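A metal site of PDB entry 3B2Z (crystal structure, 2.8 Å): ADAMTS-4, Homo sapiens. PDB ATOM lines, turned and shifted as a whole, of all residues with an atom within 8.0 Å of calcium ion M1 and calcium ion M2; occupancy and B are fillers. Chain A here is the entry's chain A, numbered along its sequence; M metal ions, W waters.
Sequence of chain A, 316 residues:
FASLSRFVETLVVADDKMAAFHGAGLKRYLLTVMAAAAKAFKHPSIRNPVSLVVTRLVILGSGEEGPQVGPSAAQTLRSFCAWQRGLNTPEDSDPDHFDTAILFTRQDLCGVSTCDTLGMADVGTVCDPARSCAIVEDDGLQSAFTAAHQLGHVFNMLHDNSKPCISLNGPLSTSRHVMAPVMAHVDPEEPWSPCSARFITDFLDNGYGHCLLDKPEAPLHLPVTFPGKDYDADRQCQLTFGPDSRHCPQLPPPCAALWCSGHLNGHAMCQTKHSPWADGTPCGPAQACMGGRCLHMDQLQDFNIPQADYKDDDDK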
ATOM      1  N   PHE A   7       2.411 -18.810 -16.389  1.00  0.00           N
ATOM      2  CA  PHE A   7       1.719 -19.958 -16.957  1.00  0.00           C
ATOM      3  C   PHE A   7       0.250 -19.593 -17.169  1.00  0.00           C
ATOM      4  O   PHE A   7      -0.404 -19.097 -16.259  1.00  0.00           O
ATOM      5  CB  PHE A   7       1.827 -21.178 -16.042  1.00  0.00           C
ATOM      6  CG  PHE A   7       3.230 -21.630 -15.761  1.00  0.00           C
ATOM      7  CD1 PHE A   7       3.952 -21.103 -14.688  1.00  0.00           C
ATOM      8  CD2 PHE A   7       3.838 -22.603 -16.563  1.00  0.00           C
ATOM      9  CE1 PHE A   7       5.254 -21.522 -14.427  1.00  0.00           C
ATOM     10  CE2 PHE A   7       5.148 -23.033 -16.305  1.00  0.00           C
ATOM     11  CZ  PHE A   7       5.853 -22.482 -15.236  1.00  0.00           C
ATOM     12  N   VAL A   8      -0.265 -19.818 -18.372  1.00  0.00           N
ATOM     13  CA  VAL A   8      -1.664 -19.533 -18.638  1.00  0.00           C
ATOM     14  C   VAL A   8      -2.440 -20.832 -18.654  1.00  0.00           C
ATOM     15  O   VAL A   8      -2.337 -21.603 -19.604  1.00  0.00           O
ATOM     16  CB  VAL A   8      -1.844 -18.763 -19.957  1.00  0.00           C
ATOM     17  CG1 VAL A   8      -3.304 -18.450 -20.189  1.00  0.00           C
ATOM     18  CG2 VAL A   8      -1.035 -17.462 -19.926  1.00  0.00           C
ATOM     19  N   GLU A   9      -3.178 -21.078 -17.576  1.00  0.00           N
ATOM     20  CA  GLU A   9      -3.914 -22.324 -17.427  1.00  0.00           C
ATOM     21  C   GLU A   9      -5.181 -22.212 -18.270  1.00  0.00           C
ATOM     22  O   GLU A   9      -6.185 -21.628 -17.845  1.00  0.00           O
ATOM     23  CB  GLU A   9      -4.273 -22.570 -15.957  1.00  0.00           C
ATOM     24  CG  GLU A   9      -3.106 -23.007 -15.055  1.00  0.00           C
ATOM     25  CD  GLU A   9      -3.509 -23.153 -13.584  1.00  0.00           C
ATOM     26  OE1 GLU A   9      -3.693 -22.142 -12.872  1.00  0.00           O
ATOM     27  OE2 GLU A   9      -3.633 -24.303 -13.114  1.00  0.00           O
ATOM     28  N   THR A  10      -5.093 -22.753 -19.480  1.00  0.00           N
ATOM     29  CA  THR A  10      -6.113 -22.578 -20.505  1.00  0.00           C
ATOM     30  C   THR A  10      -7.151 -23.693 -20.504  1.00  0.00           C
ATOM     31  O   THR A  10      -6.808 -24.871 -20.508  1.00  0.00           O
ATOM     32  CB  THR A  10      -5.469 -22.543 -21.896  1.00  0.00           C
ATOM     33  OG1 THR A  10      -4.231 -21.826 -21.823  1.00  0.00           O
ATOM     34  CG2 THR A  10      -6.372 -21.859 -22.904  1.00  0.00           C
ATOM     35  N   THR A  55      -4.906 -27.135 -19.584  1.00  0.00           N
ATOM     36  CA  THR A  55      -5.137 -27.978 -18.408  1.00  0.00           C
ATOM     37  C   THR A  55      -6.441 -28.750 -18.509  1.00  0.00           C
ATOM     38  O   THR A  55      -6.625 -29.760 -17.825  1.00  0.00           O
ATOM     39  CB  THR A  55      -5.122 -27.177 -17.062  1.00  0.00           C
ATOM     40  OG1 THR A  55      -6.247 -26.266 -17.010  1.00  0.00           O
ATOM     41  CG2 THR A  55      -3.825 -26.402 -16.888  1.00  0.00           C
ATOM     42  N   THR A  89     -13.698 -22.412 -11.072  1.00  0.00           N
ATOM     43  CA  THR A  89     -13.799 -22.535  -9.613  1.00  0.00           C
ATOM     44  C   THR A  89     -13.413 -21.218  -8.911  1.00  0.00           C
ATOM     45  O   THR A  89     -12.760 -20.374  -9.517  1.00  0.00           O
ATOM     46  CB  THR A  89     -12.919 -23.683  -9.070  1.00  0.00           C
ATOM     47  OG1 THR A  89     -11.569 -23.483  -9.512  1.00  0.00           O
ATOM     48  CG2 THR A  89     -13.426 -25.032  -9.554  1.00  0.00           C
ATOM     49  N   GLU A  91     -11.173 -20.456  -6.284  1.00  0.00           N
ATOM     50  CA  GLU A  91      -9.759 -20.182  -5.988  1.00  0.00           C
ATOM     51  C   GLU A  91      -8.829 -20.969  -6.913  1.00  0.00           C
ATOM     52  O   GLU A  91      -9.081 -22.138  -7.193  1.00  0.00           O
ATOM     53  CB  GLU A  91      -9.414 -20.480  -4.511  1.00  0.00           C
ATOM     54  CG  GLU A  91     -10.317 -19.785  -3.461  1.00  0.00           C
ATOM     55  CD  GLU A  91      -9.703 -18.552  -2.786  1.00  0.00           C
ATOM     56  OE1 GLU A  91      -9.150 -17.657  -3.482  1.00  0.00           O
ATOM     57  OE2 GLU A  91      -9.814 -18.463  -1.538  1.00  0.00           O
ATOM     58  N   ASP A  92      -7.739 -20.327  -7.350  1.00  0.00           N
ATOM     59  CA  ASP A  92      -6.765 -20.904  -8.301  1.00  0.00           C
ATOM     60  C   ASP A  92      -5.990 -22.096  -7.719  1.00  0.00           C
ATOM     61  O   ASP A  92      -4.955 -22.519  -8.257  1.00  0.00           O
ATOM     62  CB  ASP A  92      -5.786 -19.824  -8.768  1.00  0.00           C
ATOM     63  CG  ASP A  92      -5.168 -20.125 -10.135  1.00  0.00           C
ATOM     64  OD1 ASP A  92      -5.354 -21.234 -10.683  1.00  0.00           O
ATOM     65  OD2 ASP A  92      -4.463 -19.238 -10.672  1.00  0.00           O
ATOM     66  N   SER A  93      -6.497 -22.628  -6.617  1.00  0.00           N
ATOM     67  CA  SER A  93      -5.880 -23.716  -5.873  1.00  0.00           C
ATOM     68  C   SER A  93      -6.384 -25.079  -6.328  1.00  0.00           C
ATOM     69  O   SER A  93      -5.693 -26.092  -6.166  1.00  0.00           O
ATOM     70  CB  SER A  93      -6.192 -23.530  -4.406  1.00  0.00           C
ATOM     71  OG  SER A  93      -7.556 -23.163  -4.215  1.00  0.00           O
ATOM     72  N   ASP A  94      -7.592 -25.097  -6.883  1.00  0.00           N
ATOM     73  CA  ASP A  94      -8.190 -26.306  -7.444  1.00  0.00           C
ATOM     74  C   ASP A  94      -7.641 -26.547  -8.853  1.00  0.00           C
ATOM     75  O   ASP A  94      -7.739 -25.675  -9.709  1.00  0.00           O
ATOM     76  CB  ASP A  94      -9.720 -26.177  -7.468  1.00  0.00           C
ATOM     77  CG  ASP A  94     -10.430 -27.494  -7.793  1.00  0.00           C
ATOM     78  OD1 ASP A  94     -10.036 -28.177  -8.764  1.00  0.00           O
ATOM     79  OD2 ASP A  94     -11.408 -27.843  -7.083  1.00  0.00           O
ATOM     80  N   PRO A  95      -7.063 -27.735  -9.089  1.00  0.00           N
ATOM     81  CA  PRO A  95      -6.586 -28.115 -10.415  1.00  0.00           C
ATOM     82  C   PRO A  95      -7.576 -27.790 -11.545  1.00  0.00           C
ATOM     83  O   PRO A  95      -7.151 -27.566 -12.680  1.00  0.00           O
ATOM     84  CB  PRO A  95      -6.406 -29.624 -10.301  1.00  0.00           C
ATOM     85  CG  PRO A  95      -6.100 -29.867  -8.871  1.00  0.00           C
ATOM     86  CD  PRO A  95      -6.818 -28.798  -8.089  1.00  0.00           C
ATOM     87  N   ASP A  96      -8.872 -27.790 -11.235  1.00  0.00           N
ATOM     88  CA  ASP A  96      -9.909 -27.472 -12.215  1.00  0.00           C
ATOM     89  C   ASP A  96      -9.963 -25.979 -12.586  1.00  0.00           C
ATOM     90  O   ASP A  96     -10.519 -25.629 -13.625  1.00  0.00           O
ATOM     91  CB  ASP A  96     -11.280 -27.952 -11.721  1.00  0.00           C
ATOM     92  CG  ASP A  96     -11.475 -29.469 -11.848  1.00  0.00           C
ATOM     93  OD1 ASP A  96     -10.794 -30.112 -12.692  1.00  0.00           O
ATOM     94  OD2 ASP A  96     -12.321 -30.021 -11.117  1.00  0.00           O
ATOM     95  N   HIS A  97      -9.398 -25.114 -11.755  1.00  0.00           N
ATOM     96  CA  HIS A  97      -9.398 -23.693 -12.042  1.00  0.00           C
ATOM     97  C   HIS A  97      -8.528 -23.386 -13.253  1.00  0.00           C
ATOM     98  O   HIS A  97      -7.357 -23.772 -13.295  1.00  0.00           O
ATOM     99  CB  HIS A  97      -8.919 -22.853 -10.854  1.00  0.00           C
ATOM    100  CG  HIS A  97      -9.119 -21.383 -11.042  1.00  0.00           C
ATOM    101  ND1 HIS A  97     -10.100 -20.557 -10.615  1.00  0.00           N
ATOM    102  CD2 HIS A  97      -8.268 -20.602 -11.800  1.00  0.00           C
ATOM    103  CE1 HIS A  97      -9.816 -19.302 -11.103  1.00  0.00           C
ATOM    104  NE2 HIS A  97      -8.705 -19.361 -11.813  1.00  0.00           N
ATOM    105  N   PHE A  98      -9.111 -22.690 -14.215  1.00  0.00           N
ATOM    106  CA  PHE A  98      -8.369 -22.269 -15.390  1.00  0.00           C
ATOM    107  C   PHE A  98      -8.305 -20.735 -15.435  1.00  0.00           C
ATOM    108  O   PHE A  98      -9.177 -20.048 -14.892  1.00  0.00           O
ATOM    109  CB  PHE A  98      -8.993 -22.852 -16.671  1.00  0.00           C
ATOM    110  CG  PHE A  98     -10.467 -22.600 -16.797  1.00  0.00           C
ATOM    111  CD1 PHE A  98     -10.936 -21.397 -17.292  1.00  0.00           C
ATOM    112  CD2 PHE A  98     -11.390 -23.566 -16.424  1.00  0.00           C
ATOM    113  CE1 PHE A  98     -12.302 -21.138 -17.403  1.00  0.00           C
ATOM    114  CE2 PHE A  98     -12.769 -23.326 -16.525  1.00  0.00           C
ATOM    115  CZ  PHE A  98     -13.224 -22.106 -17.019  1.00  0.00           C
ATOM    116  N   ASP A  99      -7.262 -20.213 -16.078  1.00  0.00           N
ATOM    117  CA  ASP A  99      -7.039 -18.766 -16.181  1.00  0.00           C
ATOM    118  C   ASP A  99      -7.761 -18.109 -17.362  1.00  0.00           C
ATOM    119  O   ASP A  99      -8.302 -17.020 -17.219  1.00  0.00           O
ATOM    120  CB  ASP A  99      -5.529 -18.471 -16.233  1.00  0.00           C
ATOM    121  CG  ASP A  99      -4.808 -18.893 -14.954  1.00  0.00           C
ATOM    122  OD1 ASP A  99      -5.396 -18.832 -13.864  1.00  0.00           O
ATOM    123  OD2 ASP A  99      -3.624 -19.277 -15.039  1.00  0.00           O
ATOM    124  N   THR A 100      -7.748 -18.752 -18.535  1.00  0.00           N
ATOM    125  CA  THR A 100      -8.552 -18.260 -19.658  1.00  0.00           C
ATOM    126  C   THR A 100      -9.196 -19.392 -20.436  1.00  0.00           C
ATOM    127  O   THR A 100      -8.764 -20.531 -20.325  1.00  0.00           O
ATOM    128  CB  THR A 100      -7.786 -17.344 -20.629  1.00  0.00           C
ATOM    129  OG1 THR A 100      -8.706 -16.795 -21.592  1.00  0.00           O
ATOM    130  CG2 THR A 100      -6.655 -18.084 -21.342  1.00  0.00           C
ATOM    131  N   VAL A 126      -6.866 -11.145 -18.610  1.00  0.00           N
ATOM    132  CA  VAL A 126      -6.280 -12.443 -18.290  1.00  0.00           C
ATOM    133  C   VAL A 126      -6.756 -13.018 -16.965  1.00  0.00           C
ATOM    134  O   VAL A 126      -7.092 -14.201 -16.897  1.00  0.00           O
ATOM    135  CB  VAL A 126      -4.734 -12.444 -18.240  1.00  0.00           C
ATOM    136  CG1 VAL A 126      -4.205 -13.770 -18.786  1.00  0.00           C
ATOM    137  CG2 VAL A 126      -4.172 -11.292 -19.032  1.00  0.00           C
ATOM    138  N   CYS A 127      -6.759 -12.186 -15.929  1.00  0.00           N
ATOM    139  CA  CYS A 127      -7.056 -12.657 -14.574  1.00  0.00           C
ATOM    140  C   CYS A 127      -8.403 -12.225 -14.008  1.00  0.00           C
ATOM    141  O   CYS A 127      -8.637 -12.311 -12.809  1.00  0.00           O
ATOM    142  CB  CYS A 127      -5.897 -12.327 -13.627  1.00  0.00           C
ATOM    143  SG  CYS A 127      -4.391 -13.254 -14.017  1.00  0.00           S
ATOM    144  N   GLY A 209      -1.155  -9.843 -14.272  1.00  0.00           N
ATOM    145  CA  GLY A 209      -0.988 -11.288 -14.413  1.00  0.00           C
ATOM    146  C   GLY A 209      -0.615 -11.953 -13.097  1.00  0.00           C
ATOM    147  O   GLY A 209       0.335 -12.736 -13.053  1.00  0.00           O
ATOM    148  N   HIS A 210      -1.368 -11.628 -12.044  1.00  0.00           N
ATOM    149  CA  HIS A 210      -1.125 -12.136 -10.695  1.00  0.00           C
ATOM    150  C   HIS A 210      -1.540 -13.588 -10.564  1.00  0.00           C
ATOM    151  O   HIS A 210      -1.119 -14.287  -9.639  1.00  0.00           O
ATOM    152  CB  HIS A 210      -1.881 -11.294  -9.666  1.00  0.00           C
ATOM    153  CG  HIS A 210      -3.345 -11.569  -9.607  1.00  0.00           C
ATOM    154  ND1 HIS A 210      -4.278 -10.859 -10.350  1.00  0.00           N
ATOM    155  CD2 HIS A 210      -4.059 -12.465  -8.886  1.00  0.00           C
ATOM    156  CE1 HIS A 210      -5.489 -11.314 -10.080  1.00  0.00           C
ATOM    157  NE2 HIS A 210      -5.385 -12.292  -9.200  1.00  0.00           N
ATOM    158  N   CYS A 211      -2.367 -14.038 -11.497  1.00  0.00           N
ATOM    159  CA  CYS A 211      -2.974 -15.363 -11.410  1.00  0.00           C
ATOM    160  C   CYS A 211      -2.258 -16.377 -12.316  1.00  0.00           C
ATOM    161  O   CYS A 211      -2.638 -17.544 -12.392  1.00  0.00           O
ATOM    162  CB  CYS A 211      -4.469 -15.257 -11.739  1.00  0.00           C
ATOM    163  SG  CYS A 211      -4.840 -15.168 -13.489  1.00  0.00           S
ATOM    164  N   LEU A 212      -1.209 -15.914 -12.978  1.00  0.00           N
ATOM    165  CA  LEU A 212      -0.463 -16.758 -13.894  1.00  0.00           C
ATOM    166  C   LEU A 212       0.812 -17.247 -13.251  1.00  0.00           C
ATOM    167  O   LEU A 212       1.753 -17.633 -13.944  1.00  0.00           O
ATOM    168  CB  LEU A 212      -0.101 -15.962 -15.149  1.00  0.00           C
ATOM    169  CG  LEU A 212      -1.152 -15.101 -15.841  1.00  0.00           C
ATOM    170  CD1 LEU A 212      -0.491 -14.425 -17.036  1.00  0.00           C
ATOM    171  CD2 LEU A 212      -2.350 -15.937 -16.265  1.00  0.00           C
ATOM    172  N   LEU A 213       0.847 -17.239 -11.916  1.00  0.00           N
ATOM    173  CA  LEU A 213       2.085 -17.544 -11.209  1.00  0.00           C
ATOM    174  C   LEU A 213       2.111 -18.949 -10.678  1.00  0.00           C
ATOM    175  O   LEU A 213       3.201 -19.516 -10.530  1.00  0.00           O
ATOM    176  CB  LEU A 213       2.353 -16.540 -10.097  1.00  0.00           C
ATOM    177  CG  LEU A 213       3.164 -15.283 -10.471  1.00  0.00           C
ATOM    178  CD1 LEU A 213       3.368 -14.414  -9.237  1.00  0.00           C
ATOM    179  CD2 LEU A 213       4.503 -15.656 -11.089  1.00  0.00           C
ATOM    180  N   ASP A 214       0.941 -19.525 -10.402  1.00  0.00           N
ATOM    181  CA  ASP A 214       0.845 -20.937 -10.027  1.00  0.00           C
ATOM    182  C   ASP A 214       1.017 -21.865 -11.236  1.00  0.00           C
ATOM    183  O   ASP A 214       0.443 -21.642 -12.302  1.00  0.00           O
ATOM    184  CB  ASP A 214      -0.444 -21.252  -9.244  1.00  0.00           C
ATOM    185  CG  ASP A 214      -1.678 -21.328 -10.121  1.00  0.00           C
ATOM    186  OD1 ASP A 214      -2.016 -20.318 -10.777  1.00  0.00           O
ATOM    187  OD2 ASP A 214      -2.322 -22.396 -10.153  1.00  0.00           O
ATOM    188  N   LYS A 215       1.833 -22.895 -11.055  1.00  0.00           N
ATOM    189  CA  LYS A 215       2.073 -23.899 -12.092  1.00  0.00           C
ATOM    190  C   LYS A 215       1.084 -25.061 -11.942  1.00  0.00           C
ATOM    191  O   LYS A 215       0.998 -25.647 -10.851  1.00  0.00           O
ATOM    192  CB  LYS A 215       3.527 -24.377 -12.017  1.00  0.00           C
ATOM    193  CG  LYS A 215       3.975 -25.265 -13.169  1.00  0.00           C
ATOM    194  CD  LYS A 215       5.421 -25.713 -12.997  1.00  0.00           C
ATOM    195  CE  LYS A 215       5.864 -26.620 -14.152  1.00  0.00           C
ATOM    196  NZ  LYS A 215       7.322 -26.943 -14.095  1.00  0.00           N
ATOM    197  N   PRO A 216       0.351 -25.421 -13.019  1.00  0.00           N
ATOM    198  CA  PRO A 216      -0.597 -26.524 -12.928  1.00  0.00           C
ATOM    199  C   PRO A 216       0.132 -27.857 -12.810  1.00  0.00           C
ATOM    200  O   PRO A 216       1.153 -28.056 -13.476  1.00  0.00           O
ATOM    201  CB  PRO A 216      -1.332 -26.461 -14.269  1.00  0.00           C
ATOM    202  CG  PRO A 216      -0.367 -25.847 -15.204  1.00  0.00           C
ATOM    203  CD  PRO A 216       0.379 -24.833 -14.377  1.00  0.00           C
ATOM    204  N   GLU A 217      -0.385 -28.745 -11.976  1.00  0.00           N
ATOM    205  CA  GLU A 217       0.289 -30.029 -11.750  1.00  0.00           C
ATOM    206  C   GLU A 217       0.253 -30.955 -12.968  1.00  0.00           C
ATOM    207  O   GLU A 217       1.259 -31.572 -13.295  1.00  0.00           O
ATOM    208  CB  GLU A 217      -0.244 -30.699 -10.481  1.00  0.00           C
ATOM    209  CG  GLU A 217       0.164 -29.950  -9.193  1.00  0.00           C
ATOM    210  CD  GLU A 217      -0.754 -30.186  -7.974  1.00  0.00           C
ATOM    211  OE1 GLU A 217      -1.763 -30.925  -8.075  1.00  0.00           O
ATOM    212  OE2 GLU A 217      -0.447 -29.605  -6.911  1.00  0.00           O
HETATM  213 CA    CA M   1      -3.288 -19.706 -12.792  1.00  0.00          CA
HETATM  214 CA    CA M   2      -4.473 -23.348 -10.654  1.00  0.00          CA
HETATM  215  O   HOH W   1      -0.935 -20.109 -13.763  1.00  0.00           O
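The side-chain sulfur of Cys 127 forms a disulfide with the side-chain sulfur of Cys 211 (2.0 Å). A ring nitrogen (ND1) of His 97 lies within hydrogen-bond range of the backbone carbonyl oxygen of Thr 89 (2.9 Å). The backbone NH (N) of Thr 100 is in hydrogen-bond range of the backbone carbonyl oxygen (O) of Glu 9, 3.3 Å away.
Of the 27 residues printed, 5 come within 4 Å of calcium ion M1. The nearest printed residue that does not touch calcium ion M1 is Leu 212 (4.2 Å).
His 97 touches calcium ion M2 (O to CA, 3.9 Å). The nearest printed residue that does not touch calcium ion M2 is Asp 94 (4.1 Å).
O of Cys 211 is bound to calcium ion M1, 2.3 Å away. The side-chain carboxylate (OD2) of Asp 99 is bound to calcium ion M1. The side-chain carboxylate (OD1) of Asp 214 binds calcium ion M1, 2.5 Å away. Calcium ion M1 is bound by the side-chain carboxylate (OD2) of Asp 92 (2.5 Å). Calcium ion M1 is bound by OE1 of Glu 9, at 2.5 Å. The side-chain carboxylate (OD1) of Asp 99 is bound to calcium ion M1 (2.5 Å). Calcium ion M1 is bound by water W1 (2.6 Å).
Calcium ion M2 is bound by the side-chain carboxylate (OD1) of Asp 92 (2.3 Å), the side-chain carboxylate (OD2) of Asp 214 (2.4 Å), the backbone carbonyl oxygen (O) of Asp 92 (2.6 Å), the side-chain carboxylate (OE1) of Glu 9 (2.6 Å) and the side-chain carboxylate (OE2) of Glu 9 (2.8 Å).
Water W1 bridges the backbone carbonyl oxygen of Asp 214 (2.5 Å) and the backbone carbonyl oxygen of Phe 7 (2.7 Å).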
